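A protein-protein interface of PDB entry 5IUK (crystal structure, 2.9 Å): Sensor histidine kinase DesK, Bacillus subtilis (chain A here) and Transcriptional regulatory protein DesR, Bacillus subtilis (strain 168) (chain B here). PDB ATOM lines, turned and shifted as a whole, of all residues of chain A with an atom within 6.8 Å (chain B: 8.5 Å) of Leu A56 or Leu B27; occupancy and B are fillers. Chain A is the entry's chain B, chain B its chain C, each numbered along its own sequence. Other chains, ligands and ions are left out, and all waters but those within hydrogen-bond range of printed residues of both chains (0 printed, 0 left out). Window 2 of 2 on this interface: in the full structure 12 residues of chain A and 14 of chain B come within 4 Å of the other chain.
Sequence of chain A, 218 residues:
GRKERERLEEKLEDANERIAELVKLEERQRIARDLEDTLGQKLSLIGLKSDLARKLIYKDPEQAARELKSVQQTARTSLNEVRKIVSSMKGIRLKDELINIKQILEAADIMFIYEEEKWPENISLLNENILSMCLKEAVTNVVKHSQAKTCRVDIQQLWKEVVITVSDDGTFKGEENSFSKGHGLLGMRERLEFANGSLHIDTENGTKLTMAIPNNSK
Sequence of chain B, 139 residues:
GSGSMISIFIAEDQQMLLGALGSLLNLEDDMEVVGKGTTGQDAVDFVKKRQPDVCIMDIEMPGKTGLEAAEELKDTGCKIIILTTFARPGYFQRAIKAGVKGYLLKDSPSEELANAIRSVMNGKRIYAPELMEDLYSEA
Of the printed residues of chain B, Leu A52 touches Ser B23, Leu B24 and Leu B27. Printed residues of chain B within 4 Å of Lys A55: Leu B27 and Ser B110. Printed residues of chain A within 4 Å of Ser B23: Leu A52. Leu B27 touches just these residues of chain A: Leu A52, Lys A55 and Leu A56. Asp B29 touches none of the printed residues of chain A. Printed residues of chain A within 4 Å of Ser B110: Asp A51 (2.9 Å) and Lys A55 (3.4 Å). The nearest residue of chain B that does not touch Leu A56 is Ser B23 (6.5 Å).
The side-chain hydroxyl (OG) of Ser B110 lies within hydrogen-bond range of the side-chain carboxylate (OD1) of Asp A51, 2.9 Å away.
Leu A52 touches Ser B23. Leu B24 touches Leu A52 (CD2 to CA, 3.7 Å). CD1 of Leu A52 touches CD1 of Leu B27, 3.8 Å away. Leu B27 touches Lys A55 (CD1 to CB, 3.9 Å). CE of Lys A55 touches OG of Ser B110, at 3.4 Å. Leu B27 touches Leu A56 (CD1 to CD2, 3.9 Å).
The side-chain carboxylate (OD1) of Asp A51 is in salt-bridge range of the guanidinium group (NH2) of Arg A54, 3.3 Å away. The side-chain amino group (NZ) of Lys A55 is in salt-bridge range of the side-chain carboxylate (OD1) of Asp A51, at 3.9 Å.
Of the 16 printed residues of chain A, 4 touch a printed residue of chain B. Printed residues of chain A that touch a printed residue of chain B: Asp A51, Leu A52, Lys A55 and Leu A56. Hydrophobic or aromatic side chains of chain A that line the printed part of chain B: Leu A52 and Leu A56. Of the 17 printed residues of chain B, 4 touch a printed residue of chain A. Hydrophobic or aromatic side chains of chain B that line the printed part of chain A: Leu B24 and Leu B27. Among the printed residues, 7 pairs touch across the chains.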
ATOM      1  N   ASP A  51      19.513 -26.313  15.248  1.00  0.00           N
ATOM      2  CA  ASP A  51      20.560 -25.779  14.375  1.00  0.00           C
ATOM      3  C   ASP A  51      21.804 -26.625  14.515  1.00  0.00           C
ATOM      4  O   ASP A  51      22.294 -27.134  13.517  1.00  0.00           O
ATOM      5  CB  ASP A  51      20.889 -24.309  14.786  1.00  0.00           C
ATOM      6  CG  ASP A  51      21.218 -23.352  13.641  1.00  0.00           C
ATOM      7  OD1 ASP A  51      21.946 -23.770  12.692  1.00  0.00           O
ATOM      8  OD2 ASP A  51      20.771 -22.179  13.703  1.00  0.00           O
ATOM      9  N   LEU A  52      22.293 -26.799  15.758  1.00  0.00           N
ATOM     10  CA  LEU A  52      23.467 -27.590  16.081  1.00  0.00           C
ATOM     11  C   LEU A  52      23.238 -29.026  15.672  1.00  0.00           C
ATOM     12  O   LEU A  52      24.023 -29.531  14.887  1.00  0.00           O
ATOM     13  CB  LEU A  52      23.797 -27.469  17.585  1.00  0.00           C
ATOM     14  CG  LEU A  52      24.915 -28.360  18.163  1.00  0.00           C
ATOM     15  CD1 LEU A  52      26.258 -28.107  17.490  1.00  0.00           C
ATOM     16  CD2 LEU A  52      25.009 -28.204  19.664  1.00  0.00           C
ATOM     17  N   ALA A  53      22.139 -29.664  16.137  1.00  0.00           N
ATOM     18  CA  ALA A  53      21.810 -31.048  15.769  1.00  0.00           C
ATOM     19  C   ALA A  53      21.846 -31.290  14.260  1.00  0.00           C
ATOM     20  O   ALA A  53      22.360 -32.315  13.844  1.00  0.00           O
ATOM     21  CB  ALA A  53      20.463 -31.464  16.350  1.00  0.00           C
ATOM     22  N   ARG A  54      21.388 -30.327  13.446  1.00  0.00           N
ATOM     23  CA  ARG A  54      21.377 -30.420  11.981  1.00  0.00           C
ATOM     24  C   ARG A  54      22.803 -30.446  11.459  1.00  0.00           C
ATOM     25  O   ARG A  54      23.142 -31.288  10.600  1.00  0.00           O
ATOM     26  CB  ARG A  54      20.568 -29.268  11.383  1.00  0.00           C
ATOM     27  CG  ARG A  54      19.946 -29.529  10.018  1.00  0.00           C
ATOM     28  CD  ARG A  54      19.428 -28.238   9.391  1.00  0.00           C
ATOM     29  NE  ARG A  54      20.480 -27.212   9.230  1.00  0.00           N
ATOM     30  CZ  ARG A  54      20.597 -26.117   9.993  1.00  0.00           C
ATOM     31  NH1 ARG A  54      19.731 -25.886  10.976  1.00  0.00           N
ATOM     32  NH2 ARG A  54      21.585 -25.249   9.778  1.00  0.00           N
ATOM     33  N   LYS A  55      23.667 -29.582  12.050  1.00  0.00           N
ATOM     34  CA  LYS A  55      25.105 -29.494  11.726  1.00  0.00           C
ATOM     35  C   LYS A  55      25.926 -30.763  12.144  1.00  0.00           C
ATOM     36  O   LYS A  55      26.914 -31.080  11.478  1.00  0.00           O
ATOM     37  CB  LYS A  55      25.723 -28.208  12.318  1.00  0.00           C
ATOM     38  CG  LYS A  55      25.037 -26.918  11.860  1.00  0.00           C
ATOM     39  CD  LYS A  55      26.015 -25.748  11.705  1.00  0.00           C
ATOM     40  CE  LYS A  55      25.333 -24.446  11.332  1.00  0.00           C
ATOM     41  NZ  LYS A  55      24.713 -24.479   9.975  1.00  0.00           N
ATOM     42  N   LEU A  56      25.486 -31.501  13.213  1.00  0.00           N
ATOM     43  CA  LEU A  56      26.183 -32.683  13.756  1.00  0.00           C
ATOM     44  C   LEU A  56      25.697 -34.066  13.227  1.00  0.00           C
ATOM     45  O   LEU A  56      26.367 -35.066  13.498  1.00  0.00           O
ATOM     46  CB  LEU A  56      26.189 -32.674  15.293  1.00  0.00           C
ATOM     47  CG  LEU A  56      27.145 -31.686  16.014  1.00  0.00           C
ATOM     48  CD1 LEU A  56      27.778 -32.331  17.237  1.00  0.00           C
ATOM     49  CD2 LEU A  56      28.251 -31.135  15.106  1.00  0.00           C
ATOM     50  N   ILE A  57      24.587 -34.114  12.439  1.00  0.00           N
ATOM     51  CA  ILE A  57      24.059 -35.332  11.794  1.00  0.00           C
ATOM     52  C   ILE A  57      25.205 -36.191  11.226  1.00  0.00           C
ATOM     53  O   ILE A  57      25.267 -37.388  11.534  1.00  0.00           O
ATOM     54  CB  ILE A  57      23.008 -34.980  10.688  1.00  0.00           C
ATOM     55  CG1 ILE A  57      21.657 -34.652  11.302  1.00  0.00           C
ATOM     56  CG2 ILE A  57      22.859 -36.080   9.604  1.00  0.00           C
ATOM     57  CD1 ILE A  57      20.792 -33.861  10.397  1.00  0.00           C
ATOM     58  N   TYR A  58      26.112 -35.597  10.412  1.00  0.00           N
ATOM     59  CA  TYR A  58      27.194 -36.435   9.861  1.00  0.00           C
ATOM     60  C   TYR A  58      28.450 -36.461  10.722  1.00  0.00           C
ATOM     61  O   TYR A  58      29.006 -37.533  10.927  1.00  0.00           O
ATOM     62  CB  TYR A  58      27.525 -36.088   8.406  1.00  0.00           C
ATOM     63  CG  TYR A  58      26.407 -36.453   7.447  1.00  0.00           C
ATOM     64  CD1 TYR A  58      26.106 -37.787   7.168  1.00  0.00           C
ATOM     65  CD2 TYR A  58      25.645 -35.470   6.826  1.00  0.00           C
ATOM     66  CE1 TYR A  58      25.082 -38.127   6.284  1.00  0.00           C
ATOM     67  CE2 TYR A  58      24.619 -35.799   5.940  1.00  0.00           C
ATOM     68  CZ  TYR A  58      24.355 -37.130   5.653  1.00  0.00           C
ATOM     69  OH  TYR A  58      23.341 -37.447   4.776  1.00  0.00           O
ATOM     70  N   LYS A  59      28.852 -35.315  11.263  1.00  0.00           N
ATOM     71  CA  LYS A  59      30.055 -35.156  12.076  1.00  0.00           C
ATOM     72  C   LYS A  59      30.053 -36.005  13.367  1.00  0.00           C
ATOM     73  O   LYS A  59      31.030 -36.713  13.626  1.00  0.00           O
ATOM     74  CB  LYS A  59      30.307 -33.656  12.379  1.00  0.00           C
ATOM     75  CG  LYS A  59      30.181 -32.754  11.151  1.00  0.00           C
ATOM     76  CD  LYS A  59      31.133 -31.566  11.198  1.00  0.00           C
ATOM     77  CE  LYS A  59      31.384 -31.018   9.808  1.00  0.00           C
ATOM     78  NZ  LYS A  59      32.442 -29.979   9.795  1.00  0.00           N
ATOM     79  N   ASP A  60      28.973 -35.905  14.179  1.00  0.00           N
ATOM     80  CA  ASP A  60      28.770 -36.625  15.439  1.00  0.00           C
ATOM     81  C   ASP A  60      27.266 -36.913  15.610  1.00  0.00           C
ATOM     82  O   ASP A  60      26.552 -36.202  16.335  1.00  0.00           O
ATOM     83  CB  ASP A  60      29.345 -35.849  16.632  1.00  0.00           C
ATOM     84  CG  ASP A  60      29.214 -36.570  17.959  1.00  0.00           C
ATOM     85  OD1 ASP A  60      28.902 -37.791  17.954  1.00  0.00           O
ATOM     86  OD2 ASP A  60      29.427 -35.929  19.000  1.00  0.00           O
ATOM     87  N   PRO A  61      26.774 -37.956  14.900  1.00  0.00           N
ATOM     88  CA  PRO A  61      25.334 -38.281  14.939  1.00  0.00           C
ATOM     89  C   PRO A  61      24.776 -38.597  16.314  1.00  0.00           C
ATOM     90  O   PRO A  61      23.581 -38.430  16.534  1.00  0.00           O
ATOM     91  CB  PRO A  61      25.244 -39.514  14.043  1.00  0.00           C
ATOM     92  CG  PRO A  61      26.635 -40.090  14.085  1.00  0.00           C
ATOM     93  CD  PRO A  61      27.492 -38.888  14.018  1.00  0.00           C
ATOM     94  N   GLU A  62      25.635 -39.083  17.209  1.00  0.00           N
ATOM     95  CA  GLU A  62      25.312 -39.481  18.572  1.00  0.00           C
ATOM     96  C   GLU A  62      24.964 -38.245  19.408  1.00  0.00           C
ATOM     97  O   GLU A  62      24.032 -38.305  20.221  1.00  0.00           O
ATOM     98  CB  GLU A  62      26.478 -40.277  19.193  1.00  0.00           C
ATOM     99  CG  GLU A  62      27.013 -41.417  18.326  1.00  0.00           C
ATOM    100  CD  GLU A  62      26.720 -42.834  18.796  1.00  0.00           C
ATOM    101  OE1 GLU A  62      26.107 -42.996  19.879  1.00  0.00           O
ATOM    102  OE2 GLU A  62      27.115 -43.786  18.081  1.00  0.00           O
ATOM    103  N   GLN A  63      25.694 -37.119  19.178  1.00  0.00           N
ATOM    104  CA  GLN A  63      25.450 -35.842  19.859  1.00  0.00           C
ATOM    105  C   GLN A  63      24.194 -35.206  19.293  1.00  0.00           C
ATOM    106  O   GLN A  63      23.346 -34.759  20.070  1.00  0.00           O
ATOM    107  CB  GLN A  63      26.645 -34.896  19.738  1.00  0.00           C
ATOM    108  CG  GLN A  63      26.713 -33.821  20.806  1.00  0.00           C
ATOM    109  CD  GLN A  63      26.526 -34.355  22.210  1.00  0.00           C
ATOM    110  OE1 GLN A  63      27.177 -35.322  22.635  1.00  0.00           O
ATOM    111  NE2 GLN A  63      25.624 -33.728  22.961  1.00  0.00           N
ATOM    112  N   ALA A  64      24.040 -35.218  17.940  1.00  0.00           N
ATOM    113  CA  ALA A  64      22.830 -34.727  17.273  1.00  0.00           C
ATOM    114  C   ALA A  64      21.575 -35.408  17.895  1.00  0.00           C
ATOM    115  O   ALA A  64      20.608 -34.720  18.243  1.00  0.00           O
ATOM    116  CB  ALA A  64      22.904 -35.001  15.790  1.00  0.00           C
ATOM    117  N   ALA A  65      21.650 -36.729  18.137  1.00  0.00           N
ATOM    118  CA  ALA A  65      20.575 -37.491  18.760  1.00  0.00           C
ATOM    119  C   ALA A  65      20.347 -37.010  20.186  1.00  0.00           C
ATOM    120  O   ALA A  65      19.199 -36.827  20.582  1.00  0.00           O
ATOM    121  CB  ALA A  65      20.900 -38.975  18.734  1.00  0.00           C
ATOM    122  N   GLU A  67      20.962 -33.934  21.499  1.00  0.00           N
ATOM    123  CA  GLU A  67      20.412 -32.575  21.412  1.00  0.00           C
ATOM    124  C   GLU A  67      18.899 -32.625  21.140  1.00  0.00           C
ATOM    125  O   GLU A  67      18.143 -31.831  21.708  1.00  0.00           O
ATOM    126  CB  GLU A  67      21.115 -31.785  20.280  1.00  0.00           C
ATOM    127  CG  GLU A  67      22.619 -31.574  20.445  1.00  0.00           C
ATOM    128  CD  GLU A  67      23.136 -30.877  21.696  1.00  0.00           C
ATOM    129  OE1 GLU A  67      22.470 -29.945  22.211  1.00  0.00           O
ATOM    130  OE2 GLU A  67      24.246 -31.252  22.141  1.00  0.00           O
ATOM    131  N   ALA B  20      25.354 -24.457  24.159  1.00  0.00           N
ATOM    132  CA  ALA B  20      24.909 -24.566  22.763  1.00  0.00           C
ATOM    133  C   ALA B  20      25.580 -23.529  21.866  1.00  0.00           C
ATOM    134  O   ALA B  20      25.934 -23.857  20.730  1.00  0.00           O
ATOM    135  CB  ALA B  20      23.397 -24.437  22.665  1.00  0.00           C
ATOM    136  N   LEU B  21      25.779 -22.282  22.381  1.00  0.00           N
ATOM    137  CA  LEU B  21      26.427 -21.210  21.622  1.00  0.00           C
ATOM    138  C   LEU B  21      27.899 -21.524  21.369  1.00  0.00           C
ATOM    139  O   LEU B  21      28.382 -21.323  20.246  1.00  0.00           O
ATOM    140  CB  LEU B  21      26.250 -19.825  22.277  1.00  0.00           C
ATOM    141  CG  LEU B  21      24.845 -19.213  22.222  1.00  0.00           C
ATOM    142  CD1 LEU B  21      24.626 -18.145  23.324  1.00  0.00           C
ATOM    143  CD2 LEU B  21      24.543 -18.653  20.856  1.00  0.00           C
ATOM    144  N   GLY B  22      28.589 -22.036  22.398  1.00  0.00           N
ATOM    145  CA  GLY B  22      29.999 -22.416  22.317  1.00  0.00           C
ATOM    146  C   GLY B  22      30.225 -23.492  21.278  1.00  0.00           C
ATOM    147  O   GLY B  22      31.155 -23.409  20.474  1.00  0.00           O
ATOM    148  N   SER B  23      29.329 -24.487  21.277  1.00  0.00           N
ATOM    149  CA  SER B  23      29.291 -25.603  20.350  1.00  0.00           C
ATOM    150  C   SER B  23      29.045 -25.107  18.935  1.00  0.00           C
ATOM    151  O   SER B  23      29.729 -25.524  18.018  1.00  0.00           O
ATOM    152  CB  SER B  23      28.190 -26.565  20.767  1.00  0.00           C
ATOM    153  OG  SER B  23      28.380 -26.915  22.124  1.00  0.00           O
ATOM    154  N   LEU B  24      28.101 -24.187  18.775  1.00  0.00           N
ATOM    155  CA  LEU B  24      27.741 -23.627  17.491  1.00  0.00           C
ATOM    156  C   LEU B  24      28.851 -22.813  16.853  1.00  0.00           C
ATOM    157  O   LEU B  24      29.067 -22.935  15.638  1.00  0.00           O
ATOM    158  CB  LEU B  24      26.436 -22.830  17.590  1.00  0.00           C
ATOM    159  CG  LEU B  24      25.233 -23.720  17.273  1.00  0.00           C
ATOM    160  CD1 LEU B  24      23.954 -22.998  17.512  1.00  0.00           C
ATOM    161  CD2 LEU B  24      25.311 -24.340  15.838  1.00  0.00           C
ATOM    162  N   LEU B  25      29.591 -22.040  17.671  1.00  0.00           N
ATOM    163  CA  LEU B  25      30.681 -21.183  17.212  1.00  0.00           C
ATOM    164  C   LEU B  25      31.994 -21.925  17.019  1.00  0.00           C
ATOM    165  O   LEU B  25      32.724 -21.577  16.094  1.00  0.00           O
ATOM    166  CB  LEU B  25      30.848 -19.951  18.109  1.00  0.00           C
ATOM    167  CG  LEU B  25      29.676 -18.914  18.092  1.00  0.00           C
ATOM    168  CD1 LEU B  25      29.938 -17.793  19.102  1.00  0.00           C
ATOM    169  CD2 LEU B  25      29.410 -18.328  16.652  1.00  0.00           C
ATOM    170  N   ASN B  26      32.265 -22.993  17.806  1.00  0.00           N
ATOM    171  CA  ASN B  26      33.465 -23.830  17.645  1.00  0.00           C
ATOM    172  C   ASN B  26      33.465 -24.629  16.330  1.00  0.00           C
ATOM    173  O   ASN B  26      34.508 -25.147  15.917  1.00  0.00           O
ATOM    174  CB  ASN B  26      33.680 -24.733  18.867  1.00  0.00           C
ATOM    175  CG  ASN B  26      34.345 -24.026  20.021  1.00  0.00           C
ATOM    176  OD1 ASN B  26      35.330 -23.317  19.848  1.00  0.00           O
ATOM    177  ND2 ASN B  26      33.857 -24.236  21.236  1.00  0.00           N
ATOM    178  N   LEU B  27      32.303 -24.685  15.667  1.00  0.00           N
ATOM    179  CA  LEU B  27      32.085 -25.360  14.399  1.00  0.00           C
ATOM    180  C   LEU B  27      32.685 -24.591  13.222  1.00  0.00           C
ATOM    181  O   LEU B  27      33.038 -25.206  12.196  1.00  0.00           O
ATOM    182  CB  LEU B  27      30.604 -25.689  14.205  1.00  0.00           C
ATOM    183  CG  LEU B  27      30.098 -26.932  15.015  1.00  0.00           C
ATOM    184  CD1 LEU B  27      28.682 -27.333  14.622  1.00  0.00           C
ATOM    185  CD2 LEU B  27      31.027 -28.135  14.900  1.00  0.00           C
ATOM    186  N   GLU B  28      32.887 -23.267  13.412  1.00  0.00           N
ATOM    187  CA  GLU B  28      33.521 -22.381  12.451  1.00  0.00           C
ATOM    188  C   GLU B  28      35.057 -22.583  12.422  1.00  0.00           C
ATOM    189  O   GLU B  28      35.708 -22.756  13.465  1.00  0.00           O
ATOM    190  CB  GLU B  28      33.175 -20.924  12.746  1.00  0.00           C
ATOM    191  CG  GLU B  28      31.693 -20.614  12.700  1.00  0.00           C
ATOM    192  CD  GLU B  28      30.952 -20.856  11.398  1.00  0.00           C
ATOM    193  OE1 GLU B  28      31.509 -20.572  10.316  1.00  0.00           O
ATOM    194  OE2 GLU B  28      29.780 -21.284  11.463  1.00  0.00           O
ATOM    195  N   ASP B  29      35.615 -22.558  11.202  1.00  0.00           N
ATOM    196  CA  ASP B  29      37.035 -22.760  10.913  1.00  0.00           C
ATOM    197  C   ASP B  29      37.938 -21.630  11.406  1.00  0.00           C
ATOM    198  O   ASP B  29      39.061 -21.887  11.845  1.00  0.00           O
ATOM    199  CB  ASP B  29      37.220 -22.977   9.404  1.00  0.00           C
ATOM    200  CG  ASP B  29      36.725 -24.314   8.881  1.00  0.00           C
ATOM    201  OD1 ASP B  29      36.662 -25.282   9.677  1.00  0.00           O
ATOM    202  OD2 ASP B  29      36.451 -24.411   7.662  1.00  0.00           O
ATOM    203  N   ASP B  30      37.433 -20.393  11.334  1.00  0.00           N
ATOM    204  CA  ASP B  30      38.143 -19.163  11.668  1.00  0.00           C
ATOM    205  C   ASP B  30      37.766 -18.592  13.046  1.00  0.00           C
ATOM    206  O   ASP B  30      38.052 -17.426  13.315  1.00  0.00           O
ATOM    207  CB  ASP B  30      37.858 -18.126  10.566  1.00  0.00           C
ATOM    208  CG  ASP B  30      36.394 -17.686  10.426  1.00  0.00           C
ATOM    209  OD1 ASP B  30      35.492 -18.403  10.941  1.00  0.00           O
ATOM    210  OD2 ASP B  30      36.153 -16.634   9.804  1.00  0.00           O
ATOM    211  N   MET B  31      37.107 -19.392  13.893  1.00  0.00           N
ATOM    212  CA  MET B  31      36.656 -18.947  15.210  1.00  0.00           C
ATOM    213  C   MET B  31      37.044 -19.926  16.291  1.00  0.00           C
ATOM    214  O   MET B  31      37.225 -21.115  16.009  1.00  0.00           O
ATOM    215  CB  MET B  31      35.137 -18.741  15.228  1.00  0.00           C
ATOM    216  CG  MET B  31      34.703 -17.491  14.567  1.00  0.00           C
ATOM    217  SD  MET B  31      32.919 -17.382  14.441  1.00  0.00           S
ATOM    218  CE  MET B  31      32.809 -16.219  13.095  1.00  0.00           C
ATOM    219  N   GLU B  32      37.119 -19.425  17.540  1.00  0.00           N
ATOM    220  CA  GLU B  32      37.523 -20.176  18.721  1.00  0.00           C
ATOM    221  C   GLU B  32      36.921 -19.561  19.988  1.00  0.00           C
ATOM    222  O   GLU B  32      37.081 -18.360  20.239  1.00  0.00           O
ATOM    223  CB  GLU B  32      39.062 -20.158  18.804  1.00  0.00           C
ATOM    224  CG  GLU B  32      39.693 -21.094  19.822  1.00  0.00           C
ATOM    225  CD  GLU B  32      41.209 -20.989  19.937  1.00  0.00           C
ATOM    226  OE1 GLU B  32      41.799 -20.060  19.339  1.00  0.00           O
ATOM    227  OE2 GLU B  32      41.811 -21.829  20.645  1.00  0.00           O
ATOM    228  N   VAL B  33      36.252 -20.388  20.792  1.00  0.00           N
ATOM    229  CA  VAL B  33      35.693 -19.934  22.060  1.00  0.00           C
ATOM    230  C   VAL B  33      36.832 -20.132  23.075  1.00  0.00           C
ATOM    231  O   VAL B  33      37.267 -21.262  23.299  1.00  0.00           O
ATOM    232  CB  VAL B  33      34.350 -20.635  22.437  1.00  0.00           C
ATOM    233  CG1 VAL B  33      33.819 -20.149  23.789  1.00  0.00           C
ATOM    234  CG2 VAL B  33      33.297 -20.428  21.346  1.00  0.00           C
ATOM    235  N   SER B 110      22.529 -19.555  13.569  1.00  0.00           N
ATOM    236  CA  SER B 110      23.985 -19.563  13.824  1.00  0.00           C
ATOM    237  C   SER B 110      24.842 -19.033  12.655  1.00  0.00           C
ATOM    238  O   SER B 110      25.867 -18.385  12.902  1.00  0.00           O
ATOM    239  CB  SER B 110      24.451 -20.959  14.213  1.00  0.00           C
ATOM    240  OG  SER B 110      24.098 -21.910  13.220  1.00  0.00           O
ATOM    241  N   ALA B 114      27.689 -16.046  13.196  1.00  0.00           N
ATOM    242  CA  ALA B 114      29.074 -16.160  12.787  1.00  0.00           C
ATOM    243  C   ALA B 114      29.404 -15.034  11.794  1.00  0.00           C
ATOM    244  O   ALA B 114      30.467 -14.426  11.910  1.00  0.00           O
ATOM    245  CB  ALA B 114      29.318 -17.524  12.185  1.00  0.00           C
ATOM    246  N   ARG B 118      32.258 -11.873  12.024  1.00  0.00           N
ATOM    247  CA  ARG B 118      33.188 -11.516  10.942  1.00  0.00           C
ATOM    248  C   ARG B 118      33.029 -10.048  10.528  1.00  0.00           C
ATOM    249  O   ARG B 118      34.035  -9.357  10.357  1.00  0.00           O
ATOM    250  CB  ARG B 118      32.996 -12.438   9.731  1.00  0.00           C
ATOM    251  CG  ARG B 118      33.482 -13.860   9.978  1.00  0.00           C
ATOM    252  CD  ARG B 118      33.202 -14.808   8.833  1.00  0.00           C
ATOM    253  NE  ARG B 118      33.458 -16.180   9.261  1.00  0.00           N
ATOM    254  CZ  ARG B 118      32.535 -17.132   9.356  1.00  0.00           C
ATOM    255  NH1 ARG B 118      32.866 -18.345   9.767  1.00  0.00           N
ATOM    256  NH2 ARG B 118      31.275 -16.882   9.030  1.00  0.00           N
